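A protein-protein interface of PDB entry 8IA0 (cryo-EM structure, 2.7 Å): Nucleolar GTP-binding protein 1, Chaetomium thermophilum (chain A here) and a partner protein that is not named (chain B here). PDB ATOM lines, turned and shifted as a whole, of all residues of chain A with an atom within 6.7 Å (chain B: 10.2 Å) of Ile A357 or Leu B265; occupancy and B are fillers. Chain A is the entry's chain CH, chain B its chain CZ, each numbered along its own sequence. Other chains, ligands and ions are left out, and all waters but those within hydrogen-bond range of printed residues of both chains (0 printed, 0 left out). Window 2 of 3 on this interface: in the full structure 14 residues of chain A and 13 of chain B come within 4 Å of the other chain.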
ATOM      1  N   LEU A 347     -23.658  19.178  16.722  1.00  0.00           N
ATOM      2  CA  LEU A 347     -23.789  18.056  15.800  1.00  0.00           C
ATOM      3  C   LEU A 347     -24.280  16.809  16.521  1.00  0.00           C
ATOM      4  O   LEU A 347     -25.100  16.054  15.987  1.00  0.00           O
ATOM      5  CB  LEU A 347     -22.454  17.788  15.108  1.00  0.00           C
ATOM      6  CG  LEU A 347     -21.968  18.841  14.112  1.00  0.00           C
ATOM      7  CD1 LEU A 347     -20.550  18.542  13.669  1.00  0.00           C
ATOM      8  CD2 LEU A 347     -22.891  18.915  12.914  1.00  0.00           C
ATOM      9  N   GLY A 350     -28.053  17.020  17.169  1.00  0.00           N
ATOM     10  CA  GLY A 350     -28.829  16.820  15.957  1.00  0.00           C
ATOM     11  C   GLY A 350     -28.889  15.366  15.533  1.00  0.00           C
ATOM     12  O   GLY A 350     -29.906  14.904  15.009  1.00  0.00           O
ATOM     13  N   THR A 351     -27.805  14.625  15.750  1.00  0.00           N
ATOM     14  CA  THR A 351     -27.743  13.217  15.376  1.00  0.00           C
ATOM     15  C   THR A 351     -28.344  12.380  16.499  1.00  0.00           C
ATOM     16  O   THR A 351     -27.732  12.218  17.559  1.00  0.00           O
ATOM     17  CB  THR A 351     -26.304  12.801  15.093  1.00  0.00           C
ATOM     18  OG1 THR A 351     -25.785  13.580  14.009  1.00  0.00           O
ATOM     19  CG2 THR A 351     -26.240  11.328  14.724  1.00  0.00           C
ATOM     20  N   HIS A 352     -29.540  11.847  16.269  1.00  0.00           N
ATOM     21  CA  HIS A 352     -30.215  11.049  17.277  1.00  0.00           C
ATOM     22  C   HIS A 352     -29.650   9.631  17.302  1.00  0.00           C
ATOM     23  O   HIS A 352     -28.870   9.223  16.437  1.00  0.00           O
ATOM     24  CB  HIS A 352     -31.720  11.023  17.017  1.00  0.00           C
ATOM     25  CG  HIS A 352     -32.313  12.375  16.777  1.00  0.00           C
ATOM     26  ND1 HIS A 352     -33.178  12.633  15.735  1.00  0.00           N
ATOM     27  CD2 HIS A 352     -32.168  13.544  17.444  1.00  0.00           C
ATOM     28  CE1 HIS A 352     -33.539  13.903  15.769  1.00  0.00           C
ATOM     29  NE2 HIS A 352     -32.941  14.479  16.797  1.00  0.00           N
ATOM     30  N   ASN A 354     -31.309   6.853  16.879  1.00  0.00           N
ATOM     31  CA  ASN A 354     -31.892   6.024  15.832  1.00  0.00           C
ATOM     32  C   ASN A 354     -31.216   6.213  14.481  1.00  0.00           C
ATOM     33  O   ASN A 354     -31.505   5.451  13.553  1.00  0.00           O
ATOM     34  CB  ASN A 354     -33.390   6.309  15.703  1.00  0.00           C
ATOM     35  CG  ASN A 354     -33.686   7.760  15.375  1.00  0.00           C
ATOM     36  OD1 ASN A 354     -32.779   8.574  15.217  1.00  0.00           O
ATOM     37  ND2 ASN A 354     -34.968   8.090  15.269  1.00  0.00           N
ATOM     38  N   GLY A 355     -30.332   7.199  14.349  1.00  0.00           N
ATOM     39  CA  GLY A 355     -29.689   7.496  13.089  1.00  0.00           C
ATOM     40  C   GLY A 355     -30.389   8.539  12.249  1.00  0.00           C
ATOM     41  O   GLY A 355     -29.845   8.943  11.213  1.00  0.00           O
ATOM     42  N   ASN A 356     -31.572   8.989  12.657  1.00  0.00           N
ATOM     43  CA  ASN A 356     -32.298  10.012  11.918  1.00  0.00           C
ATOM     44  C   ASN A 356     -31.675  11.375  12.192  1.00  0.00           C
ATOM     45  O   ASN A 356     -31.604  11.811  13.345  1.00  0.00           O
ATOM     46  CB  ASN A 356     -33.773  10.007  12.311  1.00  0.00           C
ATOM     47  CG  ASN A 356     -34.528   8.833  11.726  1.00  0.00           C
ATOM     48  OD1 ASN A 356     -33.939   7.803  11.398  1.00  0.00           O
ATOM     49  ND2 ASN A 356     -35.840   8.982  11.589  1.00  0.00           N
ATOM     50  N   ILE A 357     -31.223  12.045  11.132  1.00  0.00           N
ATOM     51  CA  ILE A 357     -30.669  13.386  11.272  1.00  0.00           C
ATOM     52  C   ILE A 357     -31.792  14.353  11.618  1.00  0.00           C
ATOM     53  O   ILE A 357     -32.846  14.363  10.968  1.00  0.00           O
ATOM     54  CB  ILE A 357     -29.944  13.807   9.986  1.00  0.00           C
ATOM     55  CG1 ILE A 357     -28.761  12.877   9.700  1.00  0.00           C
ATOM     56  CG2 ILE A 357     -29.475  15.247  10.082  1.00  0.00           C
ATOM     57  CD1 ILE A 357     -27.990  12.454  10.934  1.00  0.00           C
ATOM     58  N   GLY A 358     -31.575  15.166  12.647  1.00  0.00           N
ATOM     59  CA  GLY A 358     -32.587  16.114  13.059  1.00  0.00           C
ATOM     60  C   GLY A 358     -32.835  17.179  12.011  1.00  0.00           C
ATOM     61  O   GLY A 358     -32.051  17.378  11.083  1.00  0.00           O
ATOM     62  N   THR A 359     -33.963  17.874  12.164  1.00  0.00           N
ATOM     63  CA  THR A 359     -34.352  18.866  11.167  1.00  0.00           C
ATOM     64  C   THR A 359     -33.376  20.036  11.140  1.00  0.00           C
ATOM     65  O   THR A 359     -32.856  20.394  10.077  1.00  0.00           O
ATOM     66  CB  THR A 359     -35.781  19.349  11.426  1.00  0.00           C
ATOM     67  OG1 THR A 359     -36.028  20.545  10.675  1.00  0.00           O
ATOM     68  CG2 THR A 359     -36.011  19.613  12.906  1.00  0.00           C
ATOM     69  N   ARG A 360     -33.085  20.621  12.306  1.00  0.00           N
ATOM     70  CA  ARG A 360     -32.185  21.770  12.354  1.00  0.00           C
ATOM     71  C   ARG A 360     -30.813  21.419  11.800  1.00  0.00           C
ATOM     72  O   ARG A 360     -30.150  22.260  11.180  1.00  0.00           O
ATOM     73  CB  ARG A 360     -32.065  22.291  13.786  1.00  0.00           C
ATOM     74  CG  ARG A 360     -33.323  22.946  14.325  1.00  0.00           C
ATOM     75  CD  ARG A 360     -33.189  24.468  14.313  1.00  0.00           C
ATOM     76  NE  ARG A 360     -32.247  25.006  15.292  1.00  0.00           N
ATOM     77  CZ  ARG A 360     -32.211  24.710  16.587  1.00  0.00           C
ATOM     78  NH1 ARG A 360     -33.133  23.951  17.157  1.00  0.00           N
ATOM     79  NH2 ARG A 360     -31.238  25.218  17.340  1.00  0.00           N
ATOM     80  N   LEU A 361     -30.366  20.184  12.020  1.00  0.00           N
ATOM     81  CA  LEU A 361     -29.126  19.733  11.400  1.00  0.00           C
ATOM     82  C   LEU A 361     -29.263  19.682   9.886  1.00  0.00           C
ATOM     83  O   LEU A 361     -28.339  20.064   9.161  1.00  0.00           O
ATOM     84  CB  LEU A 361     -28.732  18.365  11.952  1.00  0.00           C
ATOM     85  CG  LEU A 361     -27.253  18.008  11.833  1.00  0.00           C
ATOM     86  CD1 LEU A 361     -26.408  19.129  12.391  1.00  0.00           C
ATOM     87  CD2 LEU A 361     -26.974  16.711  12.562  1.00  0.00           C
ATOM     88  N   GLN A 362     -30.410  19.218   9.391  1.00  0.00           N
ATOM     89  CA  GLN A 362     -30.602  19.090   7.949  1.00  0.00           C
ATOM     90  C   GLN A 362     -30.532  20.447   7.260  1.00  0.00           C
ATOM     91  O   GLN A 362     -29.940  20.577   6.183  1.00  0.00           O
ATOM     92  CB  GLN A 362     -31.935  18.403   7.657  1.00  0.00           C
ATOM     93  CG  GLN A 362     -31.937  17.568   6.389  1.00  0.00           C
ATOM     94  CD  GLN A 362     -32.890  16.392   6.467  1.00  0.00           C
ATOM     95  OE1 GLN A 362     -33.397  16.059   7.539  1.00  0.00           O
ATOM     96  NE2 GLN A 362     -33.142  15.756   5.328  1.00  0.00           N
ATOM     97  N   MET A 365     -27.040  21.634   6.991  1.00  0.00           N
ATOM     98  CA  MET A 365     -26.294  20.903   5.972  1.00  0.00           C
ATOM     99  C   MET A 365     -26.342  21.623   4.631  1.00  0.00           C
ATOM    100  O   MET A 365     -25.333  21.695   3.920  1.00  0.00           O
ATOM    101  CB  MET A 365     -26.836  19.480   5.824  1.00  0.00           C
ATOM    102  CG  MET A 365     -26.682  18.598   7.052  1.00  0.00           C
ATOM    103  SD  MET A 365     -24.988  18.515   7.657  1.00  0.00           S
ATOM    104  CE  MET A 365     -24.433  16.999   6.881  1.00  0.00           C
ATOM    105  N   PHE B 222     -22.665   3.231   4.849  1.00  0.00           N
ATOM    106  CA  PHE B 222     -21.803   4.314   5.291  1.00  0.00           C
ATOM    107  C   PHE B 222     -22.596   5.354   6.081  1.00  0.00           C
ATOM    108  O   PHE B 222     -23.710   5.744   5.713  1.00  0.00           O
ATOM    109  CB  PHE B 222     -21.137   4.973   4.082  1.00  0.00           C
ATOM    110  CG  PHE B 222     -19.716   4.572   3.868  1.00  0.00           C
ATOM    111  CD1 PHE B 222     -19.409   3.422   3.154  1.00  0.00           C
ATOM    112  CD2 PHE B 222     -18.690   5.359   4.359  1.00  0.00           C
ATOM    113  CE1 PHE B 222     -18.114   3.054   2.951  1.00  0.00           C
ATOM    114  CE2 PHE B 222     -17.376   4.998   4.159  1.00  0.00           C
ATOM    115  CZ  PHE B 222     -17.090   3.840   3.450  1.00  0.00           C
ATOM    116  N   GLY B 223     -21.994   5.830   7.164  1.00  0.00           N
ATOM    117  CA  GLY B 223     -22.572   6.900   7.943  1.00  0.00           C
ATOM    118  C   GLY B 223     -23.566   6.480   9.004  1.00  0.00           C
ATOM    119  O   GLY B 223     -24.166   7.351   9.648  1.00  0.00           O
ATOM    120  N   LYS B 224     -23.767   5.178   9.209  1.00  0.00           N
ATOM    121  CA  LYS B 224     -24.597   4.680  10.300  1.00  0.00           C
ATOM    122  C   LYS B 224     -23.881   3.584  11.078  1.00  0.00           C
ATOM    123  O   LYS B 224     -24.504   2.606  11.497  1.00  0.00           O
ATOM    124  CB  LYS B 224     -25.946   4.173   9.790  1.00  0.00           C
ATOM    125  CG  LYS B 224     -26.833   5.248   9.184  1.00  0.00           C
ATOM    126  CD  LYS B 224     -27.975   4.645   8.373  1.00  0.00           C
ATOM    127  CE  LYS B 224     -27.492   3.757   7.235  1.00  0.00           C
ATOM    128  NZ  LYS B 224     -26.234   4.248   6.606  1.00  0.00           N
ATOM    129  N   VAL B 225     -22.571   3.736  11.278  1.00  0.00           N
ATOM    130  CA  VAL B 225     -21.788   2.702  11.948  1.00  0.00           C
ATOM    131  C   VAL B 225     -22.218   2.550  13.401  1.00  0.00           C
ATOM    132  O   VAL B 225     -22.387   1.430  13.899  1.00  0.00           O
ATOM    133  CB  VAL B 225     -20.284   3.014  11.827  1.00  0.00           C
ATOM    134  CG1 VAL B 225     -19.500   2.350  12.945  1.00  0.00           C
ATOM    135  CG2 VAL B 225     -19.765   2.569  10.471  1.00  0.00           C
ATOM    136  N   LYS B 227     -25.081   3.256  14.963  1.00  0.00           N
ATOM    137  CA  LYS B 227     -26.392   2.637  15.126  1.00  0.00           C
ATOM    138  C   LYS B 227     -26.342   1.149  14.809  1.00  0.00           C
ATOM    139  O   LYS B 227     -26.955   0.335  15.510  1.00  0.00           O
ATOM    140  CB  LYS B 227     -27.418   3.342  14.240  1.00  0.00           C
ATOM    141  CG  LYS B 227     -28.642   2.505  13.908  1.00  0.00           C
ATOM    142  CD  LYS B 227     -29.634   2.488  15.060  1.00  0.00           C
ATOM    143  CE  LYS B 227     -30.877   1.689  14.703  1.00  0.00           C
ATOM    144  NZ  LYS B 227     -31.914   1.768  15.769  1.00  0.00           N
ATOM    145  N   GLN B 253     -12.791   5.250   6.578  1.00  0.00           N
ATOM    146  CA  GLN B 253     -13.812   6.198   7.008  1.00  0.00           C
ATOM    147  C   GLN B 253     -14.867   5.560   7.905  1.00  0.00           C
ATOM    148  O   GLN B 253     -15.632   6.289   8.547  1.00  0.00           O
ATOM    149  CB  GLN B 253     -14.455   6.873   5.795  1.00  0.00           C
ATOM    150  CG  GLN B 253     -14.974   8.281   6.114  1.00  0.00           C
ATOM    151  CD  GLN B 253     -16.451   8.342   6.420  1.00  0.00           C
ATOM    152  OE1 GLN B 253     -17.297   7.880   5.629  1.00  0.00           O
ATOM    153  NE2 GLN B 253     -16.777   8.866   7.600  1.00  0.00           N
ATOM    154  N   ARG B 256     -12.957   6.435  10.806  1.00  0.00           N
ATOM    155  CA  ARG B 256     -13.145   7.866  11.025  1.00  0.00           C
ATOM    156  C   ARG B 256     -14.507   8.149  11.642  1.00  0.00           C
ATOM    157  O   ARG B 256     -14.629   9.007  12.525  1.00  0.00           O
ATOM    158  CB  ARG B 256     -12.977   8.638   9.719  1.00  0.00           C
ATOM    159  CG  ARG B 256     -11.694   8.339   8.970  1.00  0.00           C
ATOM    160  CD  ARG B 256     -10.937   9.616   8.650  1.00  0.00           C
ATOM    161  NE  ARG B 256     -11.827  10.748   8.424  1.00  0.00           N
ATOM    162  CZ  ARG B 256     -12.413  11.025   7.267  1.00  0.00           C
ATOM    163  NH1 ARG B 256     -12.218  10.273   6.196  1.00  0.00           N
ATOM    164  NH2 ARG B 256     -13.213  12.083   7.183  1.00  0.00           N
ATOM    165  N   GLU B 257     -15.540   7.439  11.189  1.00  0.00           N
ATOM    166  CA  GLU B 257     -16.860   7.574  11.797  1.00  0.00           C
ATOM    167  C   GLU B 257     -16.824   7.225  13.279  1.00  0.00           C
ATOM    168  O   GLU B 257     -17.636   7.726  14.065  1.00  0.00           O
ATOM    169  CB  GLU B 257     -17.860   6.692  11.051  1.00  0.00           C
ATOM    170  CG  GLU B 257     -19.275   6.788  11.563  1.00  0.00           C
ATOM    171  CD  GLU B 257     -20.274   6.155  10.626  1.00  0.00           C
ATOM    172  OE1 GLU B 257     -21.473   6.145  10.970  1.00  0.00           O
ATOM    173  OE2 GLU B 257     -19.865   5.678   9.547  1.00  0.00           O
ATOM    174  N   TRP B 258     -15.881   6.372  13.681  1.00  0.00           N
ATOM    175  CA  TRP B 258     -15.745   6.024  15.089  1.00  0.00           C
ATOM    176  C   TRP B 258     -15.160   7.174  15.897  1.00  0.00           C
ATOM    177  O   TRP B 258     -15.424   7.296  17.098  1.00  0.00           O
ATOM    178  CB  TRP B 258     -14.876   4.775  15.232  1.00  0.00           C
ATOM    179  CG  TRP B 258     -15.649   3.520  15.459  1.00  0.00           C
ATOM    180  CD1 TRP B 258     -16.258   2.748  14.517  1.00  0.00           C
ATOM    181  CD2 TRP B 258     -15.877   2.876  16.716  1.00  0.00           C
ATOM    182  NE1 TRP B 258     -16.866   1.669  15.111  1.00  0.00           N
ATOM    183  CE2 TRP B 258     -16.643   1.725  16.463  1.00  0.00           C
ATOM    184  CE3 TRP B 258     -15.512   3.166  18.033  1.00  0.00           C
ATOM    185  CZ2 TRP B 258     -17.052   0.863  17.475  1.00  0.00           C
ATOM    186  CZ3 TRP B 258     -15.916   2.309  19.038  1.00  0.00           C
ATOM    187  CH2 TRP B 258     -16.679   1.171  18.754  1.00  0.00           C
ATOM    188  N   TYR B 259     -14.355   8.027  15.259  1.00  0.00           N
ATOM    189  CA  TYR B 259     -13.623   9.037  16.015  1.00  0.00           C
ATOM    190  C   TYR B 259     -14.547  10.148  16.499  1.00  0.00           C
ATOM    191  O   TYR B 259     -14.419  10.620  17.634  1.00  0.00           O
ATOM    192  CB  TYR B 259     -12.493   9.617  15.165  1.00  0.00           C
ATOM    193  CG  TYR B 259     -11.358   8.650  14.929  1.00  0.00           C
ATOM    194  CD1 TYR B 259     -10.636   8.119  15.985  1.00  0.00           C
ATOM    195  CD2 TYR B 259     -10.990   8.292  13.642  1.00  0.00           C
ATOM    196  CE1 TYR B 259      -9.601   7.232  15.763  1.00  0.00           C
ATOM    197  CE2 TYR B 259      -9.954   7.414  13.411  1.00  0.00           C
ATOM    198  CZ  TYR B 259      -9.259   6.889  14.475  1.00  0.00           C
ATOM    199  OH  TYR B 259      -8.223   6.012  14.252  1.00  0.00           O
ATOM    200  N   GLY B 260     -15.478  10.582  15.654  1.00  0.00           N
ATOM    201  CA  GLY B 260     -16.389  11.640  16.014  1.00  0.00           C
ATOM    202  C   GLY B 260     -17.535  11.772  15.036  1.00  0.00           C
ATOM    203  O   GLY B 260     -17.470  11.293  13.900  1.00  0.00           O
ATOM    204  N   PRO B 261     -18.622  12.421  15.466  1.00  0.00           N
ATOM    205  CA  PRO B 261     -19.748  12.631  14.545  1.00  0.00           C
ATOM    206  C   PRO B 261     -19.450  13.607  13.420  1.00  0.00           C
ATOM    207  O   PRO B 261     -20.149  13.574  12.400  1.00  0.00           O
ATOM    208  CB  PRO B 261     -20.865  13.142  15.462  1.00  0.00           C
ATOM    209  CG  PRO B 261     -20.166  13.754  16.610  1.00  0.00           C
ATOM    210  CD  PRO B 261     -18.878  12.994  16.799  1.00  0.00           C
ATOM    211  N   GLU B 262     -18.447  14.478  13.563  1.00  0.00           N
ATOM    212  CA  GLU B 262     -18.087  15.354  12.451  1.00  0.00           C
ATOM    213  C   GLU B 262     -17.615  14.543  11.255  1.00  0.00           C
ATOM    214  O   GLU B 262     -17.984  14.832  10.111  1.00  0.00           O
ATOM    215  CB  GLU B 262     -16.997  16.363  12.848  1.00  0.00           C
ATOM    216  CG  GLU B 262     -17.140  17.143  14.172  1.00  0.00           C
ATOM    217  CD  GLU B 262     -17.297  16.287  15.415  1.00  0.00           C
ATOM    218  OE1 GLU B 262     -17.043  15.067  15.346  1.00  0.00           O
ATOM    219  OE2 GLU B 262     -17.679  16.841  16.464  1.00  0.00           O
ATOM    220  N   PHE B 263     -16.802  13.515  11.503  1.00  0.00           N
ATOM    221  CA  PHE B 263     -16.281  12.700  10.414  1.00  0.00           C
ATOM    222  C   PHE B 263     -17.377  11.874   9.757  1.00  0.00           C
ATOM    223  O   PHE B 263     -17.331  11.642   8.544  1.00  0.00           O
ATOM    224  CB  PHE B 263     -15.168  11.793  10.932  1.00  0.00           C
ATOM    225  CG  PHE B 263     -14.014  12.540  11.529  1.00  0.00           C
ATOM    226  CD1 PHE B 263     -13.182  13.307  10.734  1.00  0.00           C
ATOM    227  CD2 PHE B 263     -13.759  12.473  12.887  1.00  0.00           C
ATOM    228  CE1 PHE B 263     -12.118  13.994  11.282  1.00  0.00           C
ATOM    229  CE2 PHE B 263     -12.696  13.158  13.441  1.00  0.00           C
ATOM    230  CZ  PHE B 263     -11.874  13.919  12.637  1.00  0.00           C
ATOM    231  N   ALA B 264     -18.359  11.419  10.535  1.00  0.00           N
ATOM    232  CA  ALA B 264     -19.454  10.634   9.975  1.00  0.00           C
ATOM    233  C   ALA B 264     -20.288  11.460   9.004  1.00  0.00           C
ATOM    234  O   ALA B 264     -20.610  11.003   7.901  1.00  0.00           O
ATOM    235  CB  ALA B 264     -20.334  10.088  11.099  1.00  0.00           C
ATOM    236  N   LEU B 265     -20.647  12.679   9.401  1.00  0.00           N
ATOM    237  CA  LEU B 265     -21.569  13.481   8.607  1.00  0.00           C
ATOM    238  C   LEU B 265     -20.884  14.144   7.419  1.00  0.00           C
ATOM    239  O   LEU B 265     -21.494  14.296   6.357  1.00  0.00           O
ATOM    240  CB  LEU B 265     -22.229  14.537   9.491  1.00  0.00           C
ATOM    241  CG  LEU B 265     -23.325  14.034  10.429  1.00  0.00           C
ATOM    242  CD1 LEU B 265     -24.084  15.203  11.024  1.00  0.00           C
ATOM    243  CD2 LEU B 265     -24.269  13.091   9.702  1.00  0.00           C
ATOM    244  N   PHE B 266     -19.625  14.540   7.573  1.00  0.00           N
ATOM    245  CA  PHE B 266     -18.955  15.405   6.613  1.00  0.00           C
ATOM    246  C   PHE B 266     -17.933  14.620   5.803  1.00  0.00           C
ATOM    247  O   PHE B 266     -17.149  13.845   6.360  1.00  0.00           O
ATOM    248  CB  PHE B 266     -18.279  16.577   7.326  1.00  0.00           C
ATOM    249  CG  PHE B 266     -19.245  17.565   7.909  1.00  0.00           C
ATOM    250  CD1 PHE B 266     -20.486  17.759   7.331  1.00  0.00           C
ATOM    251  CD2 PHE B 266     -18.917  18.294   9.039  1.00  0.00           C
ATOM    252  CE1 PHE B 266     -21.380  18.664   7.864  1.00  0.00           C
ATOM    253  CE2 PHE B 266     -19.807  19.202   9.579  1.00  0.00           C
ATOM    254  CZ  PHE B 266     -21.040  19.386   8.989  1.00  0.00           C
ATOM    255  N   LYS B 267     -17.955  14.828   4.489  1.00  0.00           N
ATOM    256  CA  LYS B 267     -16.997  14.206   3.594  1.00  0.00           C
ATOM    257  C   LYS B 267     -15.637  14.888   3.760  1.00  0.00           C
ATOM    258  O   LYS B 267     -15.555  16.119   3.801  1.00  0.00           O
ATOM    259  CB  LYS B 267     -17.514  14.309   2.154  1.00  0.00           C
ATOM    260  CG  LYS B 267     -16.568  14.771   1.041  1.00  0.00           C
ATOM    261  CD  LYS B 267     -15.535  13.716   0.666  1.00  0.00           C
ATOM    262  CE  LYS B 267     -14.491  14.271  -0.289  1.00  0.00           C
ATOM    263  NZ  LYS B 267     -13.498  13.234  -0.679  1.00  0.00           N
ATOM    264  N   PRO B 268     -14.559  14.109   3.891  1.00  0.00           N
ATOM    265  CA  PRO B 268     -13.260  14.697   4.244  1.00  0.00           C
ATOM    266  C   PRO B 268     -12.795  15.737   3.235  1.00  0.00           C
ATOM    267  O   PRO B 268     -13.041  15.628   2.033  1.00  0.00           O
ATOM    268  CB  PRO B 268     -12.317  13.488   4.276  1.00  0.00           C
ATOM    269  CG  PRO B 268     -13.029  12.413   3.515  1.00  0.00           C
ATOM    270  CD  PRO B 268     -14.485  12.644   3.773  1.00  0.00           C
ATOM    271  N   GLU B 269     -12.112  16.757   3.747  1.00  0.00           N
ATOM    272  CA  GLU B 269     -11.703  17.903   2.946  1.00  0.00           C
ATOM    273  C   GLU B 269     -10.574  17.507   1.994  1.00  0.00           C
ATOM    274  O   GLU B 269     -10.164  16.346   1.916  1.00  0.00           O
ATOM    275  CB  GLU B 269     -11.306  19.061   3.857  1.00  0.00           C
ATOM    276  CG  GLU B 269     -12.301  19.328   4.977  1.00  0.00           C
ATOM    277  CD  GLU B 269     -11.931  20.538   5.811  1.00  0.00           C
ATOM    278  OE1 GLU B 269     -11.148  21.381   5.325  1.00  0.00           O
ATOM    279  OE2 GLU B 269     -12.423  20.645   6.954  1.00  0.00           O
ATOM    280  N   TYR B 295     -15.568  11.362  22.651  1.00  0.00           N
ATOM    281  CA  TYR B 295     -16.459  10.549  21.828  1.00  0.00           C
ATOM    282  C   TYR B 295     -15.918   9.136  21.667  1.00  0.00           C
ATOM    283  O   TYR B 295     -16.670   8.158  21.739  1.00  0.00           O
ATOM    284  CB  TYR B 295     -16.661  11.201  20.462  1.00  0.00           C
ATOM    285  CG  TYR B 295     -17.932  10.768  19.771  1.00  0.00           C
ATOM    286  CD1 TYR B 295     -19.174  11.139  20.264  1.00  0.00           C
ATOM    287  CD2 TYR B 295     -17.891   9.973  18.637  1.00  0.00           C
ATOM    288  CE1 TYR B 295     -20.338  10.741  19.638  1.00  0.00           C
ATOM    289  CE2 TYR B 295     -19.047   9.570  18.003  1.00  0.00           C
ATOM    290  CZ  TYR B 295     -20.269   9.956  18.508  1.00  0.00           C
ATOM    291  OH  TYR B 295     -21.426   9.556  17.880  1.00  0.00           O
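Of chain B, only Leu B265 (3.97 Å) comes within 4 Å of Ile A357. No residue of chain B comes within 4 Å of Asn A356. No residue of chain B comes within 4 Å of Gly A358. Of chain B, only Leu B265 comes within 4 Å of Leu A361. Printed residues of chain B within 4 Å of Leu A347: Glu B262. Of the printed residues of chain B, Met A365 touches Phe B266 (3.6 Å). Of the printed residues of chain A, Lys B227 touches Asn A354 (3.8 Å). Of the printed residues of chain A, Glu B262 touches Leu A347. Of the printed residues of chain A, Phe B266 touches Met A365 (3.6 Å). Gly B223 touches none of the printed residues of chain A.
N of Asn A356 lies within hydrogen-bond range of OD1 of Asn A354. The backbone carbonyl oxygen (O) of Leu A347 lies within hydrogen-bond range of the side-chain hydroxyl (OG1) of Thr A351 (3.2 Å).
Leu A347 touches Glu B262. Thr A351 touches Leu B265 (OG1 to CD1, 3.8 Å). Asn A354 touches Lys B227. Leu B265 touches Ile A357 (CD2 to CD1, 3.97 Å). Leu B265 touches Leu A361. CE of Met A365 touches CE1 of Phe B266, at 3.6 Å.
Of the 14 printed residues of chain A, 6 touch a printed residue of chain B. Hydrophobic or aromatic side chains of chain A within 4 Å of the printed part of chain B: Leu A347, Ile A357, Leu A361 and Met A365. Along chain A the printed residues that touch a printed residue of chain B span positions 347 to 365. Of the 21 printed residues of chain B, 4 touch a printed residue of chain A. Hydrophobic or aromatic side chains of chain B within 4 Å of the printed part of chain A: Leu B265 and Phe B266. Along chain B the printed residues that touch a printed residue of chain A span positions 227 to 266. Among the printed residues, 6 pairs touch across the chains.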
